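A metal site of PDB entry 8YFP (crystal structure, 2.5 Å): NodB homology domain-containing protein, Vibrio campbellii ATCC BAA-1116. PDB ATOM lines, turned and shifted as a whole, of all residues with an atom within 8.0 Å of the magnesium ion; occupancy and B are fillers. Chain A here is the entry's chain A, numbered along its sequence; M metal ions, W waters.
The backbone carbonyl oxygen (O) of Glu 137 lies within hydrogen-bond range of the backbone NH (N) of Gln 199 (2.9 Å).
Water W1 binds the magnesium ion, at 2.1 Å.
Water W2 binds the magnesium ion.
O of Gly 329 is bound to the magnesium ion (2.2 Å).
The magnesium ion is bound by O of Gly 197, 2.2 Å away.
The side-chain carboxylate (OE1) of Glu 137 binds the magnesium ion (2.3 Å).
The magnesium ion has five donor atoms within binding distance.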
ATOM      1  N   GLU A 136     -22.890 -29.376  -5.416  1.00  0.00           N
ATOM      2  CA  GLU A 136     -21.990 -28.278  -5.056  1.00  0.00           C
ATOM      3  C   GLU A 136     -20.530 -28.695  -4.934  1.00  0.00           C
ATOM      4  O   GLU A 136     -19.652 -27.821  -4.926  1.00  0.00           O
ATOM      5  CB  GLU A 136     -22.420 -27.637  -3.735  1.00  0.00           C
ATOM      6  CG  GLU A 136     -23.888 -27.218  -3.663  1.00  0.00           C
ATOM      7  CD  GLU A 136     -24.125 -25.994  -2.776  1.00  0.00           C
ATOM      8  OE1 GLU A 136     -24.568 -24.941  -3.322  1.00  0.00           O
ATOM      9  OE2 GLU A 136     -23.872 -26.061  -1.546  1.00  0.00           O
ATOM     10  N   GLU A 137     -20.251 -29.993  -4.868  1.00  0.00           N
ATOM     11  CA  GLU A 137     -18.921 -30.483  -4.553  1.00  0.00           C
ATOM     12  C   GLU A 137     -18.219 -31.205  -5.687  1.00  0.00           C
ATOM     13  O   GLU A 137     -16.991 -31.305  -5.662  1.00  0.00           O
ATOM     14  CB  GLU A 137     -18.988 -31.433  -3.349  1.00  0.00           C
ATOM     15  CG  GLU A 137     -19.528 -30.802  -2.072  1.00  0.00           C
ATOM     16  CD  GLU A 137     -18.548 -29.800  -1.438  1.00  0.00           C
ATOM     17  OE1 GLU A 137     -17.359 -29.725  -1.847  1.00  0.00           O
ATOM     18  OE2 GLU A 137     -19.001 -29.073  -0.518  1.00  0.00           O
ATOM     19  N   LEU A 138     -18.970 -31.713  -6.663  1.00  0.00           N
ATOM     20  CA  LEU A 138     -18.424 -32.570  -7.721  1.00  0.00           C
ATOM     21  C   LEU A 138     -18.910 -32.078  -9.077  1.00  0.00           C
ATOM     22  O   LEU A 138     -20.110 -31.876  -9.281  1.00  0.00           O
ATOM     23  CB  LEU A 138     -18.815 -34.028  -7.516  1.00  0.00           C
ATOM     24  CG  LEU A 138     -18.321 -34.741  -6.245  1.00  0.00           C
ATOM     25  CD1 LEU A 138     -18.934 -36.155  -6.154  1.00  0.00           C
ATOM     26  CD2 LEU A 138     -16.789 -34.774  -6.171  1.00  0.00           C
ATOM     27  N   LEU A 193     -13.842 -23.396 -10.719  1.00  0.00           N
ATOM     28  CA  LEU A 193     -14.660 -24.354  -9.974  1.00  0.00           C
ATOM     29  C   LEU A 193     -13.916 -24.877  -8.751  1.00  0.00           C
ATOM     30  O   LEU A 193     -14.519 -25.056  -7.677  1.00  0.00           O
ATOM     31  CB  LEU A 193     -15.091 -25.515 -10.869  1.00  0.00           C
ATOM     32  CG  LEU A 193     -16.054 -25.157 -12.011  1.00  0.00           C
ATOM     33  CD1 LEU A 193     -16.550 -26.435 -12.696  1.00  0.00           C
ATOM     34  CD2 LEU A 193     -17.235 -24.305 -11.524  1.00  0.00           C
ATOM     35  N   ALA A 194     -12.604 -25.122  -8.862  1.00  0.00           N
ATOM     36  CA  ALA A 194     -11.850 -25.598  -7.714  1.00  0.00           C
ATOM     37  C   ALA A 194     -11.827 -24.539  -6.616  1.00  0.00           C
ATOM     38  O   ALA A 194     -11.975 -24.858  -5.427  1.00  0.00           O
ATOM     39  CB  ALA A 194     -10.434 -25.989  -8.118  1.00  0.00           C
ATOM     40  N   LYS A 196     -14.158 -22.620  -5.953  1.00  0.00           N
ATOM     41  CA  LYS A 196     -15.454 -22.630  -5.299  1.00  0.00           C
ATOM     42  C   LYS A 196     -15.687 -23.904  -4.502  1.00  0.00           C
ATOM     43  O   LYS A 196     -16.784 -24.077  -3.971  1.00  0.00           O
ATOM     44  CB  LYS A 196     -16.586 -22.451  -6.320  1.00  0.00           C
ATOM     45  CG  LYS A 196     -16.490 -21.153  -7.096  1.00  0.00           C
ATOM     46  CD  LYS A 196     -17.801 -20.901  -7.824  1.00  0.00           C
ATOM     47  CE  LYS A 196     -18.913 -20.568  -6.812  1.00  0.00           C
ATOM     48  NZ  LYS A 196     -20.273 -20.761  -7.407  1.00  0.00           N
ATOM     49  N   GLY A 197     -14.687 -24.780  -4.387  1.00  0.00           N
ATOM     50  CA  GLY A 197     -14.819 -25.990  -3.594  1.00  0.00           C
ATOM     51  C   GLY A 197     -15.078 -27.268  -4.384  1.00  0.00           C
ATOM     52  O   GLY A 197     -15.245 -28.328  -3.774  1.00  0.00           O
ATOM     53  N   TYR A 198     -15.105 -27.209  -5.718  1.00  0.00           N
ATOM     54  CA  TYR A 198     -15.382 -28.404  -6.503  1.00  0.00           C
ATOM     55  C   TYR A 198     -14.129 -29.258  -6.635  1.00  0.00           C
ATOM     56  O   TYR A 198     -12.999 -28.778  -6.665  1.00  0.00           O
ATOM     57  CB  TYR A 198     -15.867 -28.047  -7.904  1.00  0.00           C
ATOM     58  CG  TYR A 198     -17.289 -27.557  -7.990  1.00  0.00           C
ATOM     59  CD1 TYR A 198     -18.360 -28.462  -8.103  1.00  0.00           C
ATOM     60  CD2 TYR A 198     -17.583 -26.186  -7.999  1.00  0.00           C
ATOM     61  CE1 TYR A 198     -19.669 -28.009  -8.208  1.00  0.00           C
ATOM     62  CE2 TYR A 198     -18.887 -25.728  -8.098  1.00  0.00           C
ATOM     63  CZ  TYR A 198     -19.912 -26.642  -8.202  1.00  0.00           C
ATOM     64  OH  TYR A 198     -21.193 -26.182  -8.293  1.00  0.00           O
ATOM     65  N   GLN A 199     -14.365 -30.570  -6.717  1.00  0.00           N
ATOM     66  CA  GLN A 199     -13.456 -31.466  -7.394  1.00  0.00           C
ATOM     67  C   GLN A 199     -14.030 -31.747  -8.767  1.00  0.00           C
ATOM     68  O   GLN A 199     -15.252 -31.779  -8.938  1.00  0.00           O
ATOM     69  CB  GLN A 199     -13.280 -32.789  -6.645  1.00  0.00           C
ATOM     70  CG  GLN A 199     -12.457 -32.688  -5.383  1.00  0.00           C
ATOM     71  CD  GLN A 199     -12.303 -34.036  -4.752  1.00  0.00           C
ATOM     72  OE1 GLN A 199     -11.191 -34.533  -4.533  1.00  0.00           O
ATOM     73  NE2 GLN A 199     -13.436 -34.673  -4.481  1.00  0.00           N
ATOM     74  N   THR A 326     -11.601 -36.844   2.262  1.00  0.00           N
ATOM     75  CA  THR A 326     -12.488 -35.695   2.014  1.00  0.00           C
ATOM     76  C   THR A 326     -13.355 -35.585   3.263  1.00  0.00           C
ATOM     77  O   THR A 326     -13.865 -36.636   3.729  1.00  0.00           O
ATOM     78  CB  THR A 326     -13.277 -35.821   0.707  1.00  0.00           C
ATOM     79  OG1 THR A 326     -13.806 -34.522   0.506  1.00  0.00           O
ATOM     80  CG2 THR A 326     -14.394 -36.843   0.754  1.00  0.00           C
ATOM     81  N   HIS A 327     -13.451 -34.410   3.845  1.00  0.00           N
ATOM     82  CA  HIS A 327     -14.181 -34.149   5.087  1.00  0.00           C
ATOM     83  C   HIS A 327     -15.039 -32.907   4.885  1.00  0.00           C
ATOM     84  O   HIS A 327     -14.504 -31.831   4.580  1.00  0.00           O
ATOM     85  CB  HIS A 327     -13.240 -33.934   6.277  1.00  0.00           C
ATOM     86  CG  HIS A 327     -13.951 -33.686   7.572  1.00  0.00           C
ATOM     87  ND1 HIS A 327     -14.071 -32.435   8.138  1.00  0.00           N
ATOM     88  CD2 HIS A 327     -14.613 -34.547   8.394  1.00  0.00           C
ATOM     89  CE1 HIS A 327     -14.764 -32.537   9.260  1.00  0.00           C
ATOM     90  NE2 HIS A 327     -15.097 -33.798   9.440  1.00  0.00           N
ATOM     91  N   SER A 328     -16.357 -33.044   5.102  1.00  0.00           N
ATOM     92  CA  SER A 328     -17.330 -32.008   4.754  1.00  0.00           C
ATOM     93  C   SER A 328     -16.960 -31.294   3.473  1.00  0.00           C
ATOM     94  O   SER A 328     -16.977 -30.070   3.440  1.00  0.00           O
ATOM     95  CB  SER A 328     -17.495 -30.955   5.850  1.00  0.00           C
ATOM     96  OG  SER A 328     -17.473 -31.529   7.151  1.00  0.00           O
ATOM     97  N   GLY A 329     -16.589 -32.024   2.415  1.00  0.00           N
ATOM     98  CA  GLY A 329     -16.339 -31.420   1.127  1.00  0.00           C
ATOM     99  C   GLY A 329     -14.913 -30.966   0.890  1.00  0.00           C
ATOM    100  O   GLY A 329     -14.554 -30.714  -0.267  1.00  0.00           O
ATOM    101  N   THR A 330     -14.087 -30.863   1.943  1.00  0.00           N
ATOM    102  CA  THR A 330     -12.700 -30.405   1.820  1.00  0.00           C
ATOM    103  C   THR A 330     -11.729 -31.584   1.772  1.00  0.00           C
ATOM    104  O   THR A 330     -11.889 -32.555   2.516  1.00  0.00           O
ATOM    105  CB  THR A 330     -12.334 -29.493   3.004  1.00  0.00           C
ATOM    106  OG1 THR A 330     -13.288 -28.437   3.077  1.00  0.00           O
ATOM    107  CG2 THR A 330     -10.966 -28.892   2.844  1.00  0.00           C
ATOM    108  N   VAL A 331     -10.725 -31.473   0.906  1.00  0.00           N
ATOM    109  CA  VAL A 331      -9.688 -32.502   0.749  1.00  0.00           C
ATOM    110  C   VAL A 331      -8.564 -32.244   1.746  1.00  0.00           C
ATOM    111  O   VAL A 331      -8.081 -31.114   1.876  1.00  0.00           O
ATOM    112  CB  VAL A 331      -9.130 -32.503  -0.686  1.00  0.00           C
ATOM    113  CG1 VAL A 331      -8.049 -33.552  -0.823  1.00  0.00           C
ATOM    114  CG2 VAL A 331     -10.253 -32.722  -1.712  1.00  0.00           C
ATOM    115  N   ASP A 357      -7.040 -29.213  -0.877  1.00  0.00           N
ATOM    116  CA  ASP A 357      -7.982 -28.850  -1.933  1.00  0.00           C
ATOM    117  C   ASP A 357      -7.232 -28.464  -3.205  1.00  0.00           C
ATOM    118  O   ASP A 357      -6.162 -27.834  -3.144  1.00  0.00           O
ATOM    119  CB  ASP A 357      -8.858 -27.668  -1.508  1.00  0.00           C
ATOM    120  CG  ASP A 357     -10.158 -28.078  -0.831  1.00  0.00           C
ATOM    121  OD1 ASP A 357     -10.681 -27.236  -0.065  1.00  0.00           O
ATOM    122  OD2 ASP A 357     -10.662 -29.226  -1.052  1.00  0.00           O
ATOM    123  N   PRO A 358      -7.783 -28.771  -4.378  1.00  0.00           N
ATOM    124  CA  PRO A 358      -7.125 -28.372  -5.633  1.00  0.00           C
ATOM    125  C   PRO A 358      -7.298 -26.885  -5.939  1.00  0.00           C
ATOM    126  O   PRO A 358      -6.965 -26.429  -7.044  1.00  0.00           O
ATOM    127  CB  PRO A 358      -7.823 -29.235  -6.687  1.00  0.00           C
ATOM    128  CG  PRO A 358      -9.211 -29.471  -6.112  1.00  0.00           C
ATOM    129  CD  PRO A 358      -8.990 -29.598  -4.603  1.00  0.00           C
HETATM  130 MG    MG M   1     -15.077 -29.228  -1.769  1.00  0.00          MG
HETATM  131 CA    CA M   2     -18.894 -24.157  -2.666  1.00  0.00          CA
HETATM  132  O   HOH W   1     -15.182 -30.892  -3.026  1.00  0.00           O
HETATM  133  O   HOH W   2     -13.034 -29.405  -2.496  1.00  0.00           O
